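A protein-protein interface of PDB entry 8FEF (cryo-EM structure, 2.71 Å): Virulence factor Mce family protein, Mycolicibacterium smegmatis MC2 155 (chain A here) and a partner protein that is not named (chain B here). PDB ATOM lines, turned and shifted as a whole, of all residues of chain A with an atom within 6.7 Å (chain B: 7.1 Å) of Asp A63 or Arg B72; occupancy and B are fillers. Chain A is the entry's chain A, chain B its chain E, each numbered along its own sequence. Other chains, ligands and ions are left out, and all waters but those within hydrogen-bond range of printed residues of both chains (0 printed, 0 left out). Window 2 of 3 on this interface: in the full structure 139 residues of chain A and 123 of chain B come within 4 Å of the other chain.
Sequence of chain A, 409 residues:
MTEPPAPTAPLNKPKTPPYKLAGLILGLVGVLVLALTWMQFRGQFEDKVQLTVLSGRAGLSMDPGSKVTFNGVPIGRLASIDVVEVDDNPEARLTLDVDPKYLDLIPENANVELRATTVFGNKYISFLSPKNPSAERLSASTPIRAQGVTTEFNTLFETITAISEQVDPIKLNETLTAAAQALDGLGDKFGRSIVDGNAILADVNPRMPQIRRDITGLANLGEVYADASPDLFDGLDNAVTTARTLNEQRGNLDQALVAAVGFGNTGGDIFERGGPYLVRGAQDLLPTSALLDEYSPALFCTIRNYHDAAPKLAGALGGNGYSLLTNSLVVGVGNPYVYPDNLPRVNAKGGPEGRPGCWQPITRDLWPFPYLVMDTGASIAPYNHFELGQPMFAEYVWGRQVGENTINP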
ATOM      1  N   GLY A  59     -12.267 -15.802  18.830  1.00  0.00           N
ATOM      2  CA  GLY A  59     -13.435 -16.606  18.543  1.00  0.00           C
ATOM      3  C   GLY A  59     -14.465 -15.836  17.743  1.00  0.00           C
ATOM      4  O   GLY A  59     -14.687 -14.649  17.991  1.00  0.00           O
ATOM      5  N   LEU A  60     -15.091 -16.495  16.773  1.00  0.00           N
ATOM      6  CA  LEU A  60     -16.102 -15.837  15.964  1.00  0.00           C
ATOM      7  C   LEU A  60     -17.378 -15.641  16.775  1.00  0.00           C
ATOM      8  O   LEU A  60     -17.646 -16.362  17.738  1.00  0.00           O
ATOM      9  CB  LEU A  60     -16.396 -16.651  14.705  1.00  0.00           C
ATOM     10  CG  LEU A  60     -15.204 -16.919  13.788  1.00  0.00           C
ATOM     11  CD1 LEU A  60     -15.632 -17.752  12.597  1.00  0.00           C
ATOM     12  CD2 LEU A  60     -14.572 -15.616  13.338  1.00  0.00           C
ATOM     13  N   SER A  61     -18.164 -14.639  16.371  1.00  0.00           N
ATOM     14  CA  SER A  61     -19.372 -14.231  17.092  1.00  0.00           C
ATOM     15  C   SER A  61     -19.047 -13.834  18.530  1.00  0.00           C
ATOM     16  O   SER A  61     -19.817 -14.085  19.456  1.00  0.00           O
ATOM     17  CB  SER A  61     -20.453 -15.316  17.055  1.00  0.00           C
ATOM     18  OG  SER A  61     -20.981 -15.470  15.751  1.00  0.00           O
ATOM     19  N   MET A  62     -17.884 -13.224  18.720  1.00  0.00           N
ATOM     20  CA  MET A  62     -17.487 -12.643  19.999  1.00  0.00           C
ATOM     21  C   MET A  62     -17.178 -11.175  19.739  1.00  0.00           C
ATOM     22  O   MET A  62     -16.134 -10.841  19.170  1.00  0.00           O
ATOM     23  CB  MET A  62     -16.296 -13.378  20.605  1.00  0.00           C
ATOM     24  CG  MET A  62     -15.708 -12.692  21.826  1.00  0.00           C
ATOM     25  SD  MET A  62     -15.093 -13.849  23.061  1.00  0.00           S
ATOM     26  CE  MET A  62     -16.625 -14.458  23.748  1.00  0.00           C
ATOM     27  N   ASP A  63     -18.097 -10.310  20.136  1.00  0.00           N
ATOM     28  CA  ASP A  63     -18.046  -8.878  19.897  1.00  0.00           C
ATOM     29  C   ASP A  63     -18.280  -8.159  21.215  1.00  0.00           C
ATOM     30  O   ASP A  63     -18.756  -8.767  22.180  1.00  0.00           O
ATOM     31  CB  ASP A  63     -19.107  -8.465  18.866  1.00  0.00           C
ATOM     32  CG  ASP A  63     -18.820  -9.015  17.482  1.00  0.00           C
ATOM     33  OD1 ASP A  63     -17.649  -8.961  17.049  1.00  0.00           O
ATOM     34  OD2 ASP A  63     -19.763  -9.505  16.828  1.00  0.00           O
ATOM     35  N   PRO A  64     -17.906  -6.879  21.307  1.00  0.00           N
ATOM     36  CA  PRO A  64     -18.184  -6.115  22.530  1.00  0.00           C
ATOM     37  C   PRO A  64     -19.659  -6.169  22.904  1.00  0.00           C
ATOM     38  O   PRO A  64     -20.541  -6.050  22.053  1.00  0.00           O
ATOM     39  CB  PRO A  64     -17.742  -4.698  22.164  1.00  0.00           C
ATOM     40  CG  PRO A  64     -16.656  -4.907  21.182  1.00  0.00           C
ATOM     41  CD  PRO A  64     -17.036  -6.124  20.385  1.00  0.00           C
ATOM     42  N   GLY A  65     -19.917  -6.357  24.194  1.00  0.00           N
ATOM     43  CA  GLY A  65     -21.249  -6.630  24.683  1.00  0.00           C
ATOM     44  C   GLY A  65     -21.526  -8.090  24.959  1.00  0.00           C
ATOM     45  O   GLY A  65     -22.639  -8.420  25.388  1.00  0.00           O
ATOM     46  N   SER A  66     -20.558  -8.972  24.723  1.00  0.00           N
ATOM     47  CA  SER A  66     -20.734 -10.383  25.032  1.00  0.00           C
ATOM     48  C   SER A  66     -20.702 -10.603  26.538  1.00  0.00           C
ATOM     49  O   SER A  66     -19.915  -9.982  27.257  1.00  0.00           O
ATOM     50  CB  SER A  66     -19.647 -11.216  24.357  1.00  0.00           C
ATOM     51  OG  SER A  66     -19.758 -11.154  22.947  1.00  0.00           O
ATOM     52  N   LYS A  67     -21.563 -11.498  27.011  1.00  0.00           N
ATOM     53  CA  LYS A  67     -21.692 -11.731  28.441  1.00  0.00           C
ATOM     54  C   LYS A  67     -20.475 -12.459  28.996  1.00  0.00           C
ATOM     55  O   LYS A  67     -19.977 -13.417  28.402  1.00  0.00           O
ATOM     56  CB  LYS A  67     -22.957 -12.538  28.733  1.00  0.00           C
ATOM     57  CG  LYS A  67     -24.246 -11.787  28.466  1.00  0.00           C
ATOM     58  CD  LYS A  67     -25.454 -12.670  28.702  1.00  0.00           C
ATOM     59  CE  LYS A  67     -26.745 -11.876  28.605  1.00  0.00           C
ATOM     60  NZ  LYS A  67     -26.824 -10.825  29.655  1.00  0.00           N
ATOM     61  N   LEU A  78     -18.272  -7.997  27.994  1.00  0.00           N
ATOM     62  CA  LEU A  78     -17.026  -7.764  27.281  1.00  0.00           C
ATOM     63  C   LEU A  78     -16.985  -6.334  26.758  1.00  0.00           C
ATOM     64  O   LEU A  78     -17.931  -5.872  26.115  1.00  0.00           O
ATOM     65  CB  LEU A  78     -16.889  -8.760  26.130  1.00  0.00           C
ATOM     66  CG  LEU A  78     -15.755  -8.576  25.123  1.00  0.00           C
ATOM     67  CD1 LEU A  78     -14.407  -8.633  25.803  1.00  0.00           C
ATOM     68  CD2 LEU A  78     -15.851  -9.636  24.049  1.00  0.00           C
ATOM     69  N   ALA A  79     -15.887  -5.635  27.037  1.00  0.00           N
ATOM     70  CA  ALA A  79     -15.761  -4.237  26.647  1.00  0.00           C
ATOM     71  C   ALA A  79     -15.117  -4.078  25.273  1.00  0.00           C
ATOM     72  O   ALA A  79     -15.674  -3.406  24.401  1.00  0.00           O
ATOM     73  CB  ALA A  79     -14.963  -3.465  27.700  1.00  0.00           C
ATOM     74  N   ILE A  81     -11.973  -5.915  22.294  1.00  0.00           N
ATOM     75  CA  ILE A  81     -11.062  -6.965  21.859  1.00  0.00           C
ATOM     76  C   ILE A  81      -9.971  -6.325  21.012  1.00  0.00           C
ATOM     77  O   ILE A  81     -10.240  -5.416  20.221  1.00  0.00           O
ATOM     78  CB  ILE A  81     -11.782  -8.070  21.056  1.00  0.00           C
ATOM     79  CG1 ILE A  81     -13.098  -8.457  21.722  1.00  0.00           C
ATOM     80  CG2 ILE A  81     -10.901  -9.296  20.932  1.00  0.00           C
ATOM     81  CD1 ILE A  81     -13.851  -9.519  20.976  1.00  0.00           C
ATOM     82  N   ASN A 122     -24.184 -16.284  19.751  1.00  0.00           N
ATOM     83  CA  ASN A 122     -22.839 -15.751  19.863  1.00  0.00           C
ATOM     84  C   ASN A 122     -22.083 -16.451  20.992  1.00  0.00           C
ATOM     85  O   ASN A 122     -22.587 -17.377  21.630  1.00  0.00           O
ATOM     86  CB  ASN A 122     -22.897 -14.240  20.081  1.00  0.00           C
ATOM     87  CG  ASN A 122     -23.803 -13.852  21.227  1.00  0.00           C
ATOM     88  OD1 ASN A 122     -24.732 -14.580  21.573  1.00  0.00           O
ATOM     89  ND2 ASN A 122     -23.539 -12.696  21.823  1.00  0.00           N
ATOM     90  N   LYS A 123     -20.849 -16.021  21.230  1.00  0.00           N
ATOM     91  CA  LYS A 123     -19.998 -16.622  22.245  1.00  0.00           C
ATOM     92  C   LYS A 123     -20.005 -15.796  23.528  1.00  0.00           C
ATOM     93  O   LYS A 123     -20.375 -14.620  23.539  1.00  0.00           O
ATOM     94  CB  LYS A 123     -18.562 -16.780  21.737  1.00  0.00           C
ATOM     95  CG  LYS A 123     -18.407 -17.769  20.600  1.00  0.00           C
ATOM     96  CD  LYS A 123     -16.977 -18.270  20.506  1.00  0.00           C
ATOM     97  CE  LYS A 123     -16.752 -19.055  19.227  1.00  0.00           C
ATOM     98  NZ  LYS A 123     -17.845 -20.032  18.974  1.00  0.00           N
ATOM     99  N   LEU B  67     -19.184 -13.209  -1.317  1.00  0.00           N
ATOM    100  CA  LEU B  67     -18.786 -12.240  -0.304  1.00  0.00           C
ATOM    101  C   LEU B  67     -19.079 -10.821  -0.775  1.00  0.00           C
ATOM    102  O   LEU B  67     -18.811 -10.464  -1.926  1.00  0.00           O
ATOM    103  CB  LEU B  67     -17.295 -12.383   0.008  1.00  0.00           C
ATOM    104  CG  LEU B  67     -16.670 -11.468   1.061  1.00  0.00           C
ATOM    105  CD1 LEU B  67     -17.009 -11.946   2.456  1.00  0.00           C
ATOM    106  CD2 LEU B  67     -15.169 -11.380   0.873  1.00  0.00           C
ATOM    107  N   ASN B  68     -19.647 -10.018   0.116  1.00  0.00           N
ATOM    108  CA  ASN B  68     -19.947  -8.626  -0.175  1.00  0.00           C
ATOM    109  C   ASN B  68     -18.790  -7.733   0.250  1.00  0.00           C
ATOM    110  O   ASN B  68     -17.941  -8.116   1.058  1.00  0.00           O
ATOM    111  CB  ASN B  68     -21.225  -8.180   0.536  1.00  0.00           C
ATOM    112  CG  ASN B  68     -22.474  -8.737  -0.108  1.00  0.00           C
ATOM    113  OD1 ASN B  68     -22.408  -9.621  -0.959  1.00  0.00           O
ATOM    114  ND2 ASN B  68     -23.625  -8.221   0.299  1.00  0.00           N
ATOM    115  N   ALA B  69     -18.765  -6.529  -0.310  1.00  0.00           N
ATOM    116  CA  ALA B  69     -17.842  -5.515   0.166  1.00  0.00           C
ATOM    117  C   ALA B  69     -18.238  -5.077   1.574  1.00  0.00           C
ATOM    118  O   ALA B  69     -19.328  -5.385   2.065  1.00  0.00           O
ATOM    119  CB  ALA B  69     -17.817  -4.321  -0.787  1.00  0.00           C
ATOM    120  N   ASN B  70     -17.316  -4.372   2.234  1.00  0.00           N
ATOM    121  CA  ASN B  70     -17.465  -3.916   3.617  1.00  0.00           C
ATOM    122  C   ASN B  70     -17.541  -5.076   4.604  1.00  0.00           C
ATOM    123  O   ASN B  70     -17.973  -4.896   5.745  1.00  0.00           O
ATOM    124  CB  ASN B  70     -18.679  -2.993   3.792  1.00  0.00           C
ATOM    125  CG  ASN B  70     -18.673  -1.836   2.820  1.00  0.00           C
ATOM    126  OD1 ASN B  70     -17.631  -1.243   2.552  1.00  0.00           O
ATOM    127  ND2 ASN B  70     -19.841  -1.514   2.279  1.00  0.00           N
ATOM    128  N   SER B  71     -17.131  -6.270   4.185  1.00  0.00           N
ATOM    129  CA  SER B  71     -17.021  -7.389   5.103  1.00  0.00           C
ATOM    130  C   SER B  71     -15.813  -7.196   6.014  1.00  0.00           C
ATOM    131  O   SER B  71     -14.987  -6.302   5.820  1.00  0.00           O
ATOM    132  CB  SER B  71     -16.911  -8.708   4.341  1.00  0.00           C
ATOM    133  OG  SER B  71     -18.057  -8.933   3.542  1.00  0.00           O
ATOM    134  N   ARG B  72     -15.712  -8.054   7.021  1.00  0.00           N
ATOM    135  CA  ARG B  72     -14.713  -7.899   8.066  1.00  0.00           C
ATOM    136  C   ARG B  72     -13.470  -8.725   7.770  1.00  0.00           C
ATOM    137  O   ARG B  72     -13.561  -9.914   7.444  1.00  0.00           O
ATOM    138  CB  ARG B  72     -15.287  -8.296   9.426  1.00  0.00           C
ATOM    139  CG  ARG B  72     -16.368  -7.369   9.945  1.00  0.00           C
ATOM    140  CD  ARG B  72     -16.809  -7.795  11.329  1.00  0.00           C
ATOM    141  NE  ARG B  72     -17.507  -6.731  12.041  1.00  0.00           N
ATOM    142  CZ  ARG B  72     -18.032  -6.864  13.251  1.00  0.00           C
ATOM    143  NH1 ARG B  72     -17.977  -8.012  13.905  1.00  0.00           N
ATOM    144  NH2 ARG B  72     -18.612  -5.814  13.825  1.00  0.00           N
ATOM    145  N   VAL B  73     -12.316  -8.080   7.867  1.00  0.00           N
ATOM    146  CA  VAL B  73     -11.030  -8.759   7.861  1.00  0.00           C
ATOM    147  C   VAL B  73     -10.683  -9.100   9.301  1.00  0.00           C
ATOM    148  O   VAL B  73     -10.800  -8.253  10.193  1.00  0.00           O
ATOM    149  CB  VAL B  73      -9.946  -7.885   7.212  1.00  0.00           C
ATOM    150  CG1 VAL B  73      -8.610  -8.595   7.234  1.00  0.00           C
ATOM    151  CG2 VAL B  73     -10.343  -7.545   5.794  1.00  0.00           C
ATOM    152  N   ARG B  74     -10.287 -10.344   9.536  1.00  0.00           N
ATOM    153  CA  ARG B  74     -10.070 -10.851  10.881  1.00  0.00           C
ATOM    154  C   ARG B  74      -8.678 -11.449  10.986  1.00  0.00           C
ATOM    155  O   ARG B  74      -8.288 -12.286  10.165  1.00  0.00           O
ATOM    156  CB  ARG B  74     -11.128 -11.893  11.251  1.00  0.00           C
ATOM    157  CG  ARG B  74     -12.528 -11.326  11.350  1.00  0.00           C
ATOM    158  CD  ARG B  74     -13.502 -12.361  11.859  1.00  0.00           C
ATOM    159  NE  ARG B  74     -14.849 -11.822  11.988  1.00  0.00           N
ATOM    160  CZ  ARG B  74     -15.321 -11.234  13.077  1.00  0.00           C
ATOM    161  NH1 ARG B  74     -14.575 -11.079  14.157  1.00  0.00           N
ATOM    162  NH2 ARG B  74     -16.574 -10.792  13.085  1.00  0.00           N
ATOM    163  N   ASP B  77      -9.182 -14.103  14.665  1.00  0.00           N
ATOM    164  CA  ASP B  77     -10.623 -13.944  14.846  1.00  0.00           C
ATOM    165  C   ASP B  77     -11.008 -12.558  15.342  1.00  0.00           C
ATOM    166  O   ASP B  77     -12.157 -12.347  15.743  1.00  0.00           O
ATOM    167  CB  ASP B  77     -11.202 -15.012  15.783  1.00  0.00           C
ATOM    168  CG  ASP B  77     -11.076 -16.410  15.220  1.00  0.00           C
ATOM    169  OD1 ASP B  77     -10.510 -16.562  14.118  1.00  0.00           O
ATOM    170  OD2 ASP B  77     -11.545 -17.361  15.878  1.00  0.00           O
ATOM    171  N   VAL B  78     -10.084 -11.601  15.314  1.00  0.00           N
ATOM    172  CA  VAL B  78     -10.341 -10.238  15.762  1.00  0.00           C
ATOM    173  C   VAL B  78     -10.563  -9.359  14.542  1.00  0.00           C
ATOM    174  O   VAL B  78      -9.741  -9.349  13.615  1.00  0.00           O
ATOM    175  CB  VAL B  78      -9.185  -9.704  16.625  1.00  0.00           C
ATOM    176  CG1 VAL B  78      -9.458  -8.273  17.049  1.00  0.00           C
ATOM    177  CG2 VAL B  78      -8.975 -10.585  17.838  1.00  0.00           C
ATOM    178  N   PHE B  79     -11.682  -8.639  14.541  1.00  0.00           N
ATOM    179  CA  PHE B  79     -12.064  -7.727  13.468  1.00  0.00           C
ATOM    180  C   PHE B  79     -11.115  -6.535  13.437  1.00  0.00           C
ATOM    181  O   PHE B  79     -11.178  -5.658  14.304  1.00  0.00           O
ATOM    182  CB  PHE B  79     -13.512  -7.295  13.686  1.00  0.00           C
ATOM    183  CG  PHE B  79     -13.918  -6.055  12.940  1.00  0.00           C
ATOM    184  CD1 PHE B  79     -13.703  -5.929  11.580  1.00  0.00           C
ATOM    185  CD2 PHE B  79     -14.559  -5.026  13.605  1.00  0.00           C
ATOM    186  CE1 PHE B  79     -14.097  -4.790  10.909  1.00  0.00           C
ATOM    187  CE2 PHE B  79     -14.955  -3.891  12.936  1.00  0.00           C
ATOM    188  CZ  PHE B  79     -14.725  -3.775  11.586  1.00  0.00           C
ATOM    189  N   VAL B  80     -10.230  -6.505  12.440  1.00  0.00           N
ATOM    190  CA  VAL B  80      -9.149  -5.528  12.395  1.00  0.00           C
ATOM    191  C   VAL B  80      -9.080  -4.840  11.038  1.00  0.00           C
ATOM    192  O   VAL B  80      -8.153  -4.067  10.774  1.00  0.00           O
ATOM    193  CB  VAL B  80      -7.799  -6.190  12.718  1.00  0.00           C
ATOM    194  CG1 VAL B  80      -7.760  -6.676  14.154  1.00  0.00           C
ATOM    195  CG2 VAL B  80      -7.536  -7.334  11.760  1.00  0.00           C
ATOM    196  N   GLY B  81     -10.041  -5.109  10.164  1.00  0.00           N
ATOM    197  CA  GLY B  81      -9.963  -4.516   8.842  1.00  0.00           C
ATOM    198  C   GLY B  81     -11.254  -4.680   8.073  1.00  0.00           C
ATOM    199  O   GLY B  81     -12.234  -5.241   8.566  1.00  0.00           O
ATOM    200  N   ARG B  82     -11.230  -4.193   6.835  1.00  0.00           N
ATOM    201  CA  ARG B  82     -12.403  -4.172   5.977  1.00  0.00           C
ATOM    202  C   ARG B  82     -11.980  -4.418   4.535  1.00  0.00           C
ATOM    203  O   ARG B  82     -10.908  -3.976   4.116  1.00  0.00           O
ATOM    204  CB  ARG B  82     -13.133  -2.824   6.091  1.00  0.00           C
ATOM    205  CG  ARG B  82     -14.357  -2.680   5.211  1.00  0.00           C
ATOM    206  CD  ARG B  82     -14.635  -1.222   4.900  1.00  0.00           C
ATOM    207  NE  ARG B  82     -13.480  -0.576   4.289  1.00  0.00           N
ATOM    208  CZ  ARG B  82     -13.470   0.670   3.837  1.00  0.00           C
ATOM    209  NH1 ARG B  82     -14.546   1.437   3.906  1.00  0.00           N
ATOM    210  NH2 ARG B  82     -12.356   1.157   3.303  1.00  0.00           N
ATOM    211  N   VAL B  83     -12.820  -5.125   3.782  1.00  0.00           N
ATOM    212  CA  VAL B  83     -12.599  -5.318   2.354  1.00  0.00           C
ATOM    213  C   VAL B  83     -13.303  -4.203   1.586  1.00  0.00           C
ATOM    214  O   VAL B  83     -14.488  -3.923   1.806  1.00  0.00           O
ATOM    215  CB  VAL B  83     -13.054  -6.721   1.901  1.00  0.00           C
ATOM    216  CG1 VAL B  83     -14.544  -6.939   2.099  1.00  0.00           C
ATOM    217  CG2 VAL B  83     -12.683  -6.947   0.447  1.00  0.00           C
ATOM    218  N   THR B 116     -18.841 -16.323   9.413  1.00  0.00           N
ATOM    219  CA  THR B 116     -18.815 -15.885  10.806  1.00  0.00           C
ATOM    220  C   THR B 116     -19.811 -16.664  11.659  1.00  0.00           C
ATOM    221  O   THR B 116     -19.487 -17.075  12.779  1.00  0.00           O
ATOM    222  CB  THR B 116     -19.094 -14.385  10.891  1.00  0.00           C
ATOM    223  OG1 THR B 116     -18.115 -13.672  10.128  1.00  0.00           O
ATOM    224  CG2 THR B 116     -19.031 -13.913  12.332  1.00  0.00           C
ATOM    225  N   SER B 121     -22.938 -13.560   8.823  1.00  0.00           N
ATOM    226  CA  SER B 121     -22.089 -12.912   7.841  1.00  0.00           C
ATOM    227  C   SER B 121     -20.940 -13.817   7.405  1.00  0.00           C
ATOM    228  O   SER B 121     -20.836 -14.981   7.794  1.00  0.00           O
ATOM    229  CB  SER B 121     -21.548 -11.604   8.409  1.00  0.00           C
ATOM    230  OG  SER B 121     -20.980 -11.805   9.691  1.00  0.00           O
ATOM    231  N   GLN B 122     -20.067 -13.257   6.577  1.00  0.00           N
ATOM    232  CA  GLN B 122     -18.819 -13.868   6.155  1.00  0.00           C
ATOM    233  C   GLN B 122     -17.676 -12.916   6.475  1.00  0.00           C
ATOM    234  O   GLN B 122     -17.884 -11.760   6.847  1.00  0.00           O
ATOM    235  CB  GLN B 122     -18.836 -14.197   4.660  1.00  0.00           C
ATOM    236  CG  GLN B 122     -19.924 -15.161   4.244  1.00  0.00           C
ATOM    237  CD  GLN B 122     -19.934 -15.398   2.753  1.00  0.00           C
ATOM    238  OE1 GLN B 122     -19.129 -14.830   2.020  1.00  0.00           O
ATOM    239  NE2 GLN B 122     -20.846 -16.243   2.294  1.00  0.00           N
ATOM    240  N   HIS B 123     -16.453 -13.410   6.317  1.00  0.00           N
ATOM    241  CA  HIS B 123     -15.280 -12.628   6.681  1.00  0.00           C
ATOM    242  C   HIS B 123     -14.069 -13.169   5.936  1.00  0.00           C
ATOM    243  O   HIS B 123     -14.117 -14.234   5.314  1.00  0.00           O
ATOM    244  CB  HIS B 123     -15.054 -12.652   8.195  1.00  0.00           C
ATOM    245  CG  HIS B 123     -14.806 -14.020   8.745  1.00  0.00           C
ATOM    246  ND1 HIS B 123     -15.822 -14.843   9.180  1.00  0.00           N
ATOM    247  CD2 HIS B 123     -13.658 -14.712   8.926  1.00  0.00           C
ATOM    248  CE1 HIS B 123     -15.309 -15.983   9.606  1.00  0.00           C
ATOM    249  NE2 HIS B 123     -13.998 -15.928   9.463  1.00  0.00           N
ATOM    250  N   VAL B 124     -12.975 -12.416   6.013  1.00  0.00           N
ATOM    251  CA  VAL B 124     -11.704 -12.792   5.405  1.00  0.00           C
ATOM    252  C   VAL B 124     -10.668 -12.917   6.513  1.00  0.00           C
ATOM    253  O   VAL B 124     -10.311 -11.918   7.148  1.00  0.00           O
ATOM    254  CB  VAL B 124     -11.249 -11.775   4.350  1.00  0.00           C
ATOM    255  CG1 VAL B 124      -9.937 -12.207   3.722  1.00  0.00           C
ATOM    256  CG2 VAL B 124     -12.319 -11.596   3.292  1.00  0.00           C
ATOM    257  N   GLU B 125     -10.175 -14.132   6.743  1.00  0.00           N
ATOM    258  CA  GLU B 125      -9.151 -14.387   7.743  1.00  0.00           C
ATOM    259  C   GLU B 125      -7.777 -14.185   7.125  1.00  0.00           C
ATOM    260  O   GLU B 125      -7.476 -14.759   6.075  1.00  0.00           O
ATOM    261  CB  GLU B 125      -9.263 -15.811   8.284  1.00  0.00           C
ATOM    262  CG  GLU B 125     -10.663 -16.239   8.650  1.00  0.00           C
ATOM    263  CD  GLU B 125     -10.716 -17.660   9.164  1.00  0.00           C
ATOM    264  OE1 GLU B 125      -9.680 -18.354   9.101  1.00  0.00           O
ATOM    265  OE2 GLU B 125     -11.792 -18.083   9.636  1.00  0.00           O
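Printed residues of chain A that touch a printed residue of chain B: Gly A59, Leu A60, Ser A61, Asp A63 and Ile A81.
Hydrophobic or aromatic side chains of chain A that line the printed part of chain B: Leu A60 and Ile A81.
Of the 21 printed residues of chain B, 6 touch a printed residue of chain A.
Among the printed residues, 8 pairs touch across the chains.
The side-chain hydroxyl (OG1) of Thr B116 sits at hydrogen-bond distance from a ring nitrogen (ND1) of His B123.
OG of Ser A66 sits at hydrogen-bond distance from O of Asp A63 (2.7 Å).
The backbone carbonyl oxygen (O) of Arg B72 sits at hydrogen-bond distance from the backbone NH (N) of Val B124 (2.9 Å).
NH1 of Arg B74 sits at hydrogen-bond distance from O of Asp B77, 3.2 Å away.
O of Ser A61 lies within hydrogen-bond range of N of Lys A123, 2.8 Å away.
The backbone NH of Arg B74 is in hydrogen-bond range of the backbone carbonyl oxygen of Val B124 (2.9 Å).
The backbone NH (N) of Gly A59 sits close to the side-chain carboxylate (OD2) of Asp B77 (3.4 Å).
The guanidinium group (NH1) of Arg B72 lies within salt-bridge range of the side-chain carboxylate (OD1) of Asp A63, 3.3 Å away.
Leu A60 touches Arg B74.
OD2 of Asp B77 touches N of Leu A60, 3.8 Å away.
Thr B116 touches Leu A60.
Leu A60 touches His B123.
Ser A61 touches Thr B116.
Ile A81 touches Val B78.
Printed residues of chain B within 4 Å of Leu A60: Arg B74 (3.7 Å), Asp B77 (3.8 Å), Thr B116 (3.7 Å) and His B123 (3.5 Å).
Asp A63 touches one residue of chain B.
Pro A64 touches none of the printed residues of chain B.
Of the printed residues of chain A, Val B78 touches Ile A81 (3.9 Å).
The nearest residue of chain A that does not touch Arg B72 is Met A62 (6.3 Å).
The nearest printed residue of chain A that does not touch Arg B74 is Asp A63 (4.5 Å).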
